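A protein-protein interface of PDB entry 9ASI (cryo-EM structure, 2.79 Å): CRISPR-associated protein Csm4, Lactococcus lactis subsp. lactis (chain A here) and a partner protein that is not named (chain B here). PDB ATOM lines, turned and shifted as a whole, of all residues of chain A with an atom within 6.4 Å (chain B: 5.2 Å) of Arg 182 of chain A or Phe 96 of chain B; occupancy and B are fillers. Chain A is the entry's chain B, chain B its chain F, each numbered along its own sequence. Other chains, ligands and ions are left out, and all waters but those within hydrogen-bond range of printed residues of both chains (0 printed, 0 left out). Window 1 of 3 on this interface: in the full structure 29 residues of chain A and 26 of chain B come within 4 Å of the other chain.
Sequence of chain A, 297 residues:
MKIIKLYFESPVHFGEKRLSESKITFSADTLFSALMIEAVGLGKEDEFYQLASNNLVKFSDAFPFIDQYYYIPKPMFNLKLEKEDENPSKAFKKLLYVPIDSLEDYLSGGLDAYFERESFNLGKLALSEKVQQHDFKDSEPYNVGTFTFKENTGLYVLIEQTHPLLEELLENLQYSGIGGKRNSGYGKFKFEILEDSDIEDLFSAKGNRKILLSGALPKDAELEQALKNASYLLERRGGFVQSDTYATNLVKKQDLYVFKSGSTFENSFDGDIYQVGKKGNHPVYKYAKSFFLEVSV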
ATOM      1  N   ILE A  37      -9.106 -14.721 -22.898  1.00  0.00           N
ATOM      2  CA  ILE A  37      -9.675 -15.951 -22.359  1.00  0.00           C
ATOM      3  C   ILE A  37     -11.082 -16.166 -22.902  1.00  0.00           C
ATOM      4  O   ILE A  37     -11.455 -17.282 -23.284  1.00  0.00           O
ATOM      5  CB  ILE A  37      -9.642 -15.919 -20.821  1.00  0.00           C
ATOM      6  CG1 ILE A  37      -8.205 -16.115 -20.337  1.00  0.00           C
ATOM      7  CG2 ILE A  37     -10.543 -16.991 -20.245  1.00  0.00           C
ATOM      8  CD1 ILE A  37      -7.906 -15.500 -19.007  1.00  0.00           C
ATOM      9  N   GLU A  38     -11.875 -15.096 -22.982  1.00  0.00           N
ATOM     10  CA  GLU A  38     -13.202 -15.230 -23.577  1.00  0.00           C
ATOM     11  C   GLU A  38     -13.114 -15.651 -25.038  1.00  0.00           C
ATOM     12  O   GLU A  38     -13.842 -16.549 -25.477  1.00  0.00           O
ATOM     13  CB  GLU A  38     -13.978 -13.921 -23.449  1.00  0.00           C
ATOM     14  CG  GLU A  38     -14.322 -13.556 -22.028  1.00  0.00           C
ATOM     15  CD  GLU A  38     -15.202 -14.590 -21.360  1.00  0.00           C
ATOM     16  OE1 GLU A  38     -16.019 -15.223 -22.055  1.00  0.00           O
ATOM     17  OE2 GLU A  38     -15.070 -14.780 -20.136  1.00  0.00           O
ATOM     18  N   TYR A 175     -20.578 -12.608 -17.724  1.00  0.00           N
ATOM     19  CA  TYR A 175     -20.998 -13.817 -17.040  1.00  0.00           C
ATOM     20  C   TYR A 175     -19.837 -14.685 -16.592  1.00  0.00           C
ATOM     21  O   TYR A 175     -20.066 -15.773 -16.056  1.00  0.00           O
ATOM     22  CB  TYR A 175     -21.931 -14.616 -17.949  1.00  0.00           C
ATOM     23  CG  TYR A 175     -23.052 -13.772 -18.505  1.00  0.00           C
ATOM     24  CD1 TYR A 175     -24.141 -13.429 -17.720  1.00  0.00           C
ATOM     25  CD2 TYR A 175     -23.009 -13.299 -19.808  1.00  0.00           C
ATOM     26  CE1 TYR A 175     -25.159 -12.652 -18.216  1.00  0.00           C
ATOM     27  CE2 TYR A 175     -24.023 -12.522 -20.310  1.00  0.00           C
ATOM     28  CZ  TYR A 175     -25.097 -12.202 -19.513  1.00  0.00           C
ATOM     29  OH  TYR A 175     -26.114 -11.424 -20.012  1.00  0.00           O
ATOM     30  N   SER A 176     -18.602 -14.243 -16.801  1.00  0.00           N
ATOM     31  CA  SER A 176     -17.437 -14.937 -16.277  1.00  0.00           C
ATOM     32  C   SER A 176     -16.666 -14.109 -15.262  1.00  0.00           C
ATOM     33  O   SER A 176     -15.635 -14.569 -14.766  1.00  0.00           O
ATOM     34  CB  SER A 176     -16.512 -15.359 -17.421  1.00  0.00           C
ATOM     35  OG  SER A 176     -16.028 -14.234 -18.122  1.00  0.00           O
ATOM     36  N   GLY A 177     -17.133 -12.909 -14.940  1.00  0.00           N
ATOM     37  CA  GLY A 177     -16.492 -12.088 -13.936  1.00  0.00           C
ATOM     38  C   GLY A 177     -15.139 -11.558 -14.354  1.00  0.00           C
ATOM     39  O   GLY A 177     -14.555 -12.026 -15.334  1.00  0.00           O
ATOM     40  N   ILE A 178     -14.634 -10.572 -13.625  1.00  0.00           N
ATOM     41  CA  ILE A 178     -13.306 -10.026 -13.861  1.00  0.00           C
ATOM     42  C   ILE A 178     -12.627  -9.832 -12.514  1.00  0.00           C
ATOM     43  O   ILE A 178     -13.263  -9.418 -11.540  1.00  0.00           O
ATOM     44  CB  ILE A 178     -13.364  -8.713 -14.679  1.00  0.00           C
ATOM     45  CG1 ILE A 178     -11.967  -8.298 -15.149  1.00  0.00           C
ATOM     46  CG2 ILE A 178     -14.026  -7.593 -13.896  1.00  0.00           C
ATOM     47  CD1 ILE A 178     -11.966  -7.514 -16.430  1.00  0.00           C
ATOM     48  N   GLY A 179     -11.344 -10.177 -12.447  1.00  0.00           N
ATOM     49  CA  GLY A 179     -10.582 -10.018 -11.224  1.00  0.00           C
ATOM     50  C   GLY A 179     -10.120 -11.316 -10.590  1.00  0.00           C
ATOM     51  O   GLY A 179     -10.012 -12.344 -11.262  1.00  0.00           O
ATOM     52  N   GLY A 180      -9.841 -11.275  -9.291  1.00  0.00           N
ATOM     53  CA  GLY A 180      -9.268 -12.417  -8.613  1.00  0.00           C
ATOM     54  C   GLY A 180     -10.186 -13.595  -8.374  1.00  0.00           C
ATOM     55  O   GLY A 180     -10.063 -14.612  -9.051  1.00  0.00           O
ATOM     56  N   LYS A 181     -11.121 -13.486  -7.441  1.00  0.00           N
ATOM     57  CA  LYS A 181     -11.947 -14.633  -7.070  1.00  0.00           C
ATOM     58  C   LYS A 181     -13.283 -14.594  -7.807  1.00  0.00           C
ATOM     59  O   LYS A 181     -14.356 -14.604  -7.212  1.00  0.00           O
ATOM     60  CB  LYS A 181     -12.140 -14.675  -5.560  1.00  0.00           C
ATOM     61  CG  LYS A 181     -10.856 -14.869  -4.782  1.00  0.00           C
ATOM     62  CD  LYS A 181     -10.221 -16.208  -5.089  1.00  0.00           C
ATOM     63  CE  LYS A 181     -10.605 -17.255  -4.070  1.00  0.00           C
ATOM     64  NZ  LYS A 181      -9.686 -18.419  -4.112  1.00  0.00           N
ATOM     65  N   ARG A 182     -13.199 -14.566  -9.136  1.00  0.00           N
ATOM     66  CA  ARG A 182     -14.400 -14.372  -9.937  1.00  0.00           C
ATOM     67  C   ARG A 182     -15.276 -15.615  -9.961  1.00  0.00           C
ATOM     68  O   ARG A 182     -16.502 -15.498 -10.041  1.00  0.00           O
ATOM     69  CB  ARG A 182     -14.028 -13.959 -11.356  1.00  0.00           C
ATOM     70  CG  ARG A 182     -13.049 -14.883 -12.013  1.00  0.00           C
ATOM     71  CD  ARG A 182     -12.506 -14.285 -13.277  1.00  0.00           C
ATOM     72  NE  ARG A 182     -11.876 -15.288 -14.121  1.00  0.00           N
ATOM     73  CZ  ARG A 182     -12.534 -16.196 -14.827  1.00  0.00           C
ATOM     74  NH1 ARG A 182     -13.854 -16.252 -14.820  1.00  0.00           N
ATOM     75  NH2 ARG A 182     -11.850 -17.069 -15.559  1.00  0.00           N
ATOM     76  N   ASN A 183     -14.679 -16.807  -9.909  1.00  0.00           N
ATOM     77  CA  ASN A 183     -15.492 -18.017  -9.852  1.00  0.00           C
ATOM     78  C   ASN A 183     -16.099 -18.206  -8.473  1.00  0.00           C
ATOM     79  O   ASN A 183     -17.143 -18.851  -8.341  1.00  0.00           O
ATOM     80  CB  ASN A 183     -14.665 -19.230 -10.252  1.00  0.00           C
ATOM     81  CG  ASN A 183     -14.588 -19.406 -11.747  1.00  0.00           C
ATOM     82  OD1 ASN A 183     -15.550 -19.140 -12.463  1.00  0.00           O
ATOM     83  ND2 ASN A 183     -13.437 -19.846 -12.232  1.00  0.00           N
ATOM     84  N   SER A 184     -15.460 -17.667  -7.441  1.00  0.00           N
ATOM     85  CA  SER A 184     -16.150 -17.391  -6.194  1.00  0.00           C
ATOM     86  C   SER A 184     -17.047 -16.167  -6.381  1.00  0.00           C
ATOM     87  O   SER A 184     -17.149 -15.597  -7.467  1.00  0.00           O
ATOM     88  CB  SER A 184     -15.149 -17.181  -5.065  1.00  0.00           C
ATOM     89  OG  SER A 184     -15.753 -16.506  -3.979  1.00  0.00           O
ATOM     90  N   GLY A 185     -17.696 -15.734  -5.317  1.00  0.00           N
ATOM     91  CA  GLY A 185     -18.728 -14.741  -5.513  1.00  0.00           C
ATOM     92  C   GLY A 185     -18.280 -13.304  -5.671  1.00  0.00           C
ATOM     93  O   GLY A 185     -18.923 -12.404  -5.123  1.00  0.00           O
ATOM     94  N   TYR A 186     -17.212 -13.045  -6.424  1.00  0.00           N
ATOM     95  CA  TYR A 186     -16.635 -11.705  -6.421  1.00  0.00           C
ATOM     96  C   TYR A 186     -16.700 -11.000  -7.767  1.00  0.00           C
ATOM     97  O   TYR A 186     -17.274  -9.912  -7.846  1.00  0.00           O
ATOM     98  CB  TYR A 186     -15.203 -11.775  -5.889  1.00  0.00           C
ATOM     99  CG  TYR A 186     -15.209 -12.012  -4.405  1.00  0.00           C
ATOM    100  CD1 TYR A 186     -15.927 -11.180  -3.565  1.00  0.00           C
ATOM    101  CD2 TYR A 186     -14.547 -13.091  -3.847  1.00  0.00           C
ATOM    102  CE1 TYR A 186     -15.962 -11.394  -2.214  1.00  0.00           C
ATOM    103  CE2 TYR A 186     -14.571 -13.314  -2.490  1.00  0.00           C
ATOM    104  CZ  TYR A 186     -15.281 -12.460  -1.677  1.00  0.00           C
ATOM    105  OH  TYR A 186     -15.317 -12.667  -0.320  1.00  0.00           O
ATOM    106  N   GLY A 187     -16.144 -11.565  -8.834  1.00  0.00           N
ATOM    107  CA  GLY A 187     -16.161 -10.887 -10.116  1.00  0.00           C
ATOM    108  C   GLY A 187     -17.558 -10.897 -10.704  1.00  0.00           C
ATOM    109  O   GLY A 187     -18.120 -11.977 -10.948  1.00  0.00           O
ATOM    110  N   LYS A 188     -18.147  -9.716 -10.911  1.00  0.00           N
ATOM    111  CA  LYS A 188     -19.462  -9.623 -11.542  1.00  0.00           C
ATOM    112  C   LYS A 188     -19.788  -8.189 -11.939  1.00  0.00           C
ATOM    113  O   LYS A 188     -19.708  -7.284 -11.105  1.00  0.00           O
ATOM    114  CB  LYS A 188     -20.552 -10.155 -10.612  1.00  0.00           C
ATOM    115  CG  LYS A 188     -21.891 -10.347 -11.294  1.00  0.00           C
ATOM    116  CD  LYS A 188     -23.033 -10.289 -10.304  1.00  0.00           C
ATOM    117  CE  LYS A 188     -24.312 -10.813 -10.918  1.00  0.00           C
ATOM    118  NZ  LYS A 188     -24.638 -10.099 -12.179  1.00  0.00           N
ATOM    119  N   GLN A 242      -2.983 -18.090 -16.184  1.00  0.00           N
ATOM    120  CA  GLN A 242      -4.308 -18.618 -15.869  1.00  0.00           C
ATOM    121  C   GLN A 242      -4.838 -19.355 -17.088  1.00  0.00           C
ATOM    122  O   GLN A 242      -5.528 -18.787 -17.937  1.00  0.00           O
ATOM    123  CB  GLN A 242      -5.249 -17.502 -15.440  1.00  0.00           C
ATOM    124  CG  GLN A 242      -6.617 -17.980 -14.989  1.00  0.00           C
ATOM    125  CD  GLN A 242      -7.670 -16.907 -15.092  1.00  0.00           C
ATOM    126  OE1 GLN A 242      -8.343 -16.784 -16.111  1.00  0.00           O
ATOM    127  NE2 GLN A 242      -7.819 -16.120 -14.038  1.00  0.00           N
ATOM    128  N   GLY B  46     -20.666 -16.154  -2.113  1.00  0.00           N
ATOM    129  CA  GLY B  46     -20.658 -17.194  -3.122  1.00  0.00           C
ATOM    130  C   GLY B  46     -19.686 -18.307  -2.797  1.00  0.00           C
ATOM    131  O   GLY B  46     -19.903 -19.456  -3.181  1.00  0.00           O
ATOM    132  N   LEU B  49     -21.639 -20.742  -0.204  1.00  0.00           N
ATOM    133  CA  LEU B  49     -22.591 -21.596  -0.904  1.00  0.00           C
ATOM    134  C   LEU B  49     -21.877 -22.583  -1.814  1.00  0.00           C
ATOM    135  O   LEU B  49     -22.215 -23.772  -1.841  1.00  0.00           O
ATOM    136  CB  LEU B  49     -23.569 -20.743  -1.712  1.00  0.00           C
ATOM    137  CG  LEU B  49     -24.516 -21.529  -2.622  1.00  0.00           C
ATOM    138  CD1 LEU B  49     -25.511 -22.311  -1.790  1.00  0.00           C
ATOM    139  CD2 LEU B  49     -25.232 -20.625  -3.603  1.00  0.00           C
ATOM    140  N   LYS B  50     -20.875 -22.110  -2.558  1.00  0.00           N
ATOM    141  CA  LYS B  50     -20.134 -22.977  -3.464  1.00  0.00           C
ATOM    142  C   LYS B  50     -19.446 -24.101  -2.706  1.00  0.00           C
ATOM    143  O   LYS B  50     -19.508 -25.263  -3.112  1.00  0.00           O
ATOM    144  CB  LYS B  50     -19.114 -22.148  -4.243  1.00  0.00           C
ATOM    145  CG  LYS B  50     -17.940 -22.928  -4.796  1.00  0.00           C
ATOM    146  CD  LYS B  50     -16.875 -21.984  -5.319  1.00  0.00           C
ATOM    147  CE  LYS B  50     -15.951 -22.692  -6.287  1.00  0.00           C
ATOM    148  NZ  LYS B  50     -15.262 -21.752  -7.204  1.00  0.00           N
ATOM    149  N   MET B  53     -22.070 -26.605  -1.156  1.00  0.00           N
ATOM    150  CA  MET B  53     -22.653 -27.417  -2.216  1.00  0.00           C
ATOM    151  C   MET B  53     -21.640 -28.411  -2.779  1.00  0.00           C
ATOM    152  O   MET B  53     -21.984 -29.568  -3.048  1.00  0.00           O
ATOM    153  CB  MET B  53     -23.196 -26.502  -3.311  1.00  0.00           C
ATOM    154  CG  MET B  53     -23.932 -27.200  -4.426  1.00  0.00           C
ATOM    155  SD  MET B  53     -24.629 -26.003  -5.573  1.00  0.00           S
ATOM    156  CE  MET B  53     -24.972 -27.049  -6.977  1.00  0.00           C
ATOM    157  N   PHE B  81     -16.774 -27.370 -10.365  1.00  0.00           N
ATOM    158  CA  PHE B  81     -16.271 -26.354  -9.453  1.00  0.00           C
ATOM    159  C   PHE B  81     -14.829 -25.950  -9.717  1.00  0.00           C
ATOM    160  O   PHE B  81     -14.379 -24.947  -9.154  1.00  0.00           O
ATOM    161  CB  PHE B  81     -16.389 -26.832  -7.995  1.00  0.00           C
ATOM    162  CG  PHE B  81     -17.769 -27.282  -7.613  1.00  0.00           C
ATOM    163  CD1 PHE B  81     -18.724 -26.369  -7.211  1.00  0.00           C
ATOM    164  CD2 PHE B  81     -18.109 -28.621  -7.660  1.00  0.00           C
ATOM    165  CE1 PHE B  81     -19.991 -26.783  -6.867  1.00  0.00           C
ATOM    166  CE2 PHE B  81     -19.371 -29.040  -7.317  1.00  0.00           C
ATOM    167  CZ  PHE B  81     -20.314 -28.122  -6.920  1.00  0.00           C
ATOM    168  N   ARG B  91     -10.756 -25.944 -15.202  1.00  0.00           N
ATOM    169  CA  ARG B  91     -10.890 -24.518 -14.904  1.00  0.00           C
ATOM    170  C   ARG B  91     -12.097 -24.224 -14.017  1.00  0.00           C
ATOM    171  O   ARG B  91     -11.939 -23.883 -12.839  1.00  0.00           O
ATOM    172  CB  ARG B  91     -10.973 -23.719 -16.210  1.00  0.00           C
ATOM    173  CG  ARG B  91     -11.807 -24.361 -17.299  1.00  0.00           C
ATOM    174  CD  ARG B  91     -12.045 -23.381 -18.432  1.00  0.00           C
ATOM    175  NE  ARG B  91     -12.540 -22.104 -17.935  1.00  0.00           N
ATOM    176  CZ  ARG B  91     -13.810 -21.858 -17.645  1.00  0.00           C
ATOM    177  NH1 ARG B  91     -14.749 -22.771 -17.826  1.00  0.00           N
ATOM    178  NH2 ARG B  91     -14.146 -20.664 -17.164  1.00  0.00           N
ATOM    179  N   LEU B  94     -19.159 -23.697 -13.151  1.00  0.00           N
ATOM    180  CA  LEU B  94     -19.981 -22.863 -12.295  1.00  0.00           C
ATOM    181  C   LEU B  94     -19.190 -21.648 -11.844  1.00  0.00           C
ATOM    182  O   LEU B  94     -18.007 -21.743 -11.515  1.00  0.00           O
ATOM    183  CB  LEU B  94     -20.475 -23.646 -11.081  1.00  0.00           C
ATOM    184  CG  LEU B  94     -21.526 -24.715 -11.353  1.00  0.00           C
ATOM    185  CD1 LEU B  94     -22.045 -25.282 -10.049  1.00  0.00           C
ATOM    186  CD2 LEU B  94     -22.652 -24.129 -12.175  1.00  0.00           C
ATOM    187  N   LYS B  95     -19.859 -20.500 -11.837  1.00  0.00           N
ATOM    188  CA  LYS B  95     -19.282 -19.228 -11.420  1.00  0.00           C
ATOM    189  C   LYS B  95     -20.249 -18.635 -10.402  1.00  0.00           C
ATOM    190  O   LYS B  95     -21.212 -17.955 -10.766  1.00  0.00           O
ATOM    191  CB  LYS B  95     -19.068 -18.323 -12.611  1.00  0.00           C
ATOM    192  CG  LYS B  95     -18.261 -17.091 -12.325  1.00  0.00           C
ATOM    193  CD  LYS B  95     -19.182 -15.924 -12.152  1.00  0.00           C
ATOM    194  CE  LYS B  95     -18.447 -14.634 -12.243  1.00  0.00           C
ATOM    195  NZ  LYS B  95     -19.361 -13.497 -11.989  1.00  0.00           N
ATOM    196  N   PHE B  96     -19.998 -18.917  -9.128  1.00  0.00           N
ATOM    197  CA  PHE B  96     -20.896 -18.494  -8.067  1.00  0.00           C
ATOM    198  C   PHE B  96     -20.750 -17.002  -7.810  1.00  0.00           C
ATOM    199  O   PHE B  96     -19.700 -16.407  -8.056  1.00  0.00           O
ATOM    200  CB  PHE B  96     -20.616 -19.279  -6.784  1.00  0.00           C
ATOM    201  CG  PHE B  96     -20.979 -20.736  -6.868  1.00  0.00           C
ATOM    202  CD1 PHE B  96     -20.201 -21.620  -7.596  1.00  0.00           C
ATOM    203  CD2 PHE B  96     -22.095 -21.222  -6.211  1.00  0.00           C
ATOM    204  CE1 PHE B  96     -20.534 -22.947  -7.668  1.00  0.00           C
ATOM    205  CE2 PHE B  96     -22.429 -22.554  -6.280  1.00  0.00           C
ATOM    206  CZ  PHE B  96     -21.650 -23.417  -7.011  1.00  0.00           C
ATOM    207  N   ASN B  97     -21.822 -16.397  -7.309  1.00  0.00           N
ATOM    208  CA  ASN B  97     -21.863 -14.972  -7.028  1.00  0.00           C
ATOM    209  C   ASN B  97     -22.258 -14.756  -5.576  1.00  0.00           C
ATOM    210  O   ASN B  97     -22.889 -15.615  -4.957  1.00  0.00           O
ATOM    211  CB  ASN B  97     -22.851 -14.248  -7.947  1.00  0.00           C
ATOM    212  CG  ASN B  97     -22.402 -14.238  -9.390  1.00  0.00           C
ATOM    213  OD1 ASN B  97     -23.202 -14.427 -10.302  1.00  0.00           O
ATOM    214  ND2 ASN B  97     -21.117 -14.014  -9.602  1.00  0.00           N
ATOM    215  N   ASP B  98     -21.868 -13.608  -5.030  1.00  0.00           N
ATOM    216  CA  ASP B  98     -22.336 -13.229  -3.705  1.00  0.00           C
ATOM    217  C   ASP B  98     -23.828 -12.934  -3.756  1.00  0.00           C
ATOM    218  O   ASP B  98     -24.317 -12.282  -4.682  1.00  0.00           O
ATOM    219  CB  ASP B  98     -21.569 -12.014  -3.186  1.00  0.00           C
ATOM    220  CG  ASP B  98     -20.307 -12.396  -2.440  1.00  0.00           C
ATOM    221  OD1 ASP B  98     -19.753 -13.476  -2.721  1.00  0.00           O
ATOM    222  OD2 ASP B  98     -19.863 -11.618  -1.571  1.00  0.00           O
ATOM    223  N   GLU B 147     -27.822 -15.863  -8.436  1.00  0.00           N
ATOM    224  CA  GLU B 147     -27.524 -16.165  -9.826  1.00  0.00           C
ATOM    225  C   GLU B 147     -26.243 -16.975  -9.871  1.00  0.00           C
ATOM    226  O   GLU B 147     -25.275 -16.651  -9.180  1.00  0.00           O
ATOM    227  CB  GLU B 147     -27.361 -14.894 -10.665  1.00  0.00           C
ATOM    228  CG  GLU B 147     -28.662 -14.209 -11.040  1.00  0.00           C
ATOM    229  CD  GLU B 147     -28.460 -12.756 -11.410  1.00  0.00           C
ATOM    230  OE1 GLU B 147     -27.378 -12.214 -11.106  1.00  0.00           O
ATOM    231  OE2 GLU B 147     -29.378 -12.155 -12.003  1.00  0.00           O
ATOM    232  N   ILE B 148     -26.238 -18.028 -10.681  1.00  0.00           N
ATOM    233  CA  ILE B 148     -25.055 -18.856 -10.878  1.00  0.00           C
ATOM    234  C   ILE B 148     -24.797 -18.936 -12.372  1.00  0.00           C
ATOM    235  O   ILE B 148     -25.660 -19.395 -13.129  1.00  0.00           O
ATOM    236  CB  ILE B 148     -25.216 -20.263 -10.280  1.00  0.00           C
ATOM    237  CG1 ILE B 148     -25.449 -20.177  -8.774  1.00  0.00           C
ATOM    238  CG2 ILE B 148     -23.989 -21.101 -10.562  1.00  0.00           C
ATOM    239  CD1 ILE B 148     -25.685 -21.509  -8.122  1.00  0.00           C
ATOM    240  N   PHE B 149     -23.619 -18.493 -12.797  1.00  0.00           N
ATOM    241  CA  PHE B 149     -23.262 -18.509 -14.206  1.00  0.00           C
ATOM    242  C   PHE B 149     -22.582 -19.826 -14.550  1.00  0.00           C
ATOM    243  O   PHE B 149     -21.629 -20.237 -13.884  1.00  0.00           O
ATOM    244  CB  PHE B 149     -22.351 -17.331 -14.545  1.00  0.00           C
ATOM    245  CG  PHE B 149     -22.935 -15.997 -14.194  1.00  0.00           C
ATOM    246  CD1 PHE B 149     -24.287 -15.758 -14.336  1.00  0.00           C
ATOM    247  CD2 PHE B 149     -22.130 -14.978 -13.725  1.00  0.00           C
ATOM    248  CE1 PHE B 149     -24.825 -14.532 -14.008  1.00  0.00           C
ATOM    249  CE2 PHE B 149     -22.665 -13.753 -13.398  1.00  0.00           C
ATOM    250  CZ  PHE B 149     -24.012 -13.532 -13.540  1.00  0.00           C
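Of the 17 printed residues of chain A, 10 touch a printed residue of chain B.
Printed residues of chain A that touch a printed residue of chain B: Tyr 175, Ser 176, Gly 177, Arg 182, Asn 183, Ser 184, Gly 185, Tyr 186, Gly 187 and Lys 188.
Hydrophobic or aromatic side chains of chain B within 4 Å of the printed part of chain A: Phe 96 and Phe 149.
Along chain B the printed residues that touch a printed residue of chain A span positions 46 to 149.
Of chain B, only Lys 95 (3.1 Å) and Phe 96 (3.9 Å) come within 4 Å of Arg 182 of chain A.
Of chain A, only Arg 182 (3.9 Å), Asn 183 (3.0 Å), Ser 184 (2.7 Å) and Gly 185 (3.2 Å) come within 4 Å of Phe 96 of chain B.
Of the printed residues of chain A, Gly 46 of chain B touches Gly 185.
Printed residues of chain B within 4 Å of Gly 187 of chain A: Lys 95 (2.2 Å) and Asn 97 (3.9 Å).
Of the printed residues of chain A, Asp 98 of chain B touches Gly 185 (2.8 Å) and Tyr 186 (3.96 Å).
Of the printed residues of chain B, Lys 188 of chain A touches Lys 95, Asn 97, Glu 147 and Phe 149.
Glu 38 of chain A touches none of the printed residues of chain B.
Gln 242 of chain A touches none of the printed residues of chain B.
The nearest residue of chain B that does not touch Arg 182 of chain A is Arg 91 of chain B (4.6 Å).
The side-chain amino group of Lys 95 of chain B sits close to the side-chain amide nitrogen of Asn 97 of chain B, at 3.0 Å.
The side-chain carboxylate of Asp 98 of chain B is in hydrogen-bond range of the backbone NH of Gly 46 of chain B, at 2.9 Å.
O of Ser 176 of chain A is in hydrogen-bond range of NH1 of Arg 182 of chain A (2.5 Å).
O of Glu 147 of chain B sits close to OD1 of Asn 97 of chain B.
The backbone carbonyl oxygen (O) of Phe 149 of chain B sits at hydrogen-bond distance from the backbone NH (N) of Lys 95 of chain B (2.7 Å).
O of Lys 181 of chain A lies close to N of Tyr 186 of chain A (3.3 Å).
Ser 176 of chain A touches Lys 95 of chain B (C to CE, 3.5 Å).
Gly 177 of chain A touches Lys 95 of chain B.
Asn 183 of chain A touches Lys 50 of chain B (O to NZ, 3.6 Å).
O of Leu 94 of chain B touches OD1 of Asn 183 of chain A, 3.7 Å away.
Asn 183 of chain A touches Lys 95 of chain B (OD1 to CG, 3.4 Å).
Gly 185 of chain A touches Asn 97 of chain B.
OD2 of Asp 98 of chain B touches CE1 of Tyr 186 of chain A (3.96 Å).
O of Gly 187 of chain A touches ND2 of Asn 97 of chain B, 3.9 Å away.
CB of Lys 188 of chain A touches NZ of Lys 95 of chain B, at 3.8 Å.
Asn 97 of chain B touches Lys 188 of chain A (OD1 to CE, 3.8 Å).
The side-chain carboxylate (OE1) of Glu 147 of chain B lies within salt-bridge range of the side-chain amino group (NZ) of Lys 188 of chain A (3.6 Å).
The backbone carbonyl oxygen (O) of Gly 185 of chain A sits close to the backbone NH (N) of Asp 98 of chain B (3.2 Å).
O of Asn 183 of chain A sits at hydrogen-bond distance from N of Phe 96 of chain B, at 3.0 Å.
The backbone carbonyl oxygen of Phe 96 of chain B lies close to the backbone NH of Gly 185 of chain A (3.5 Å).
The backbone carbonyl oxygen (O) of Ser 184 of chain A sits close to the backbone carbonyl oxygen (O) of Phe 96 of chain B (2.7 Å).
The backbone carbonyl oxygen of Gly 187 of chain A lies close to the side-chain amino group of Lys 95 of chain B, at 2.2 Å.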
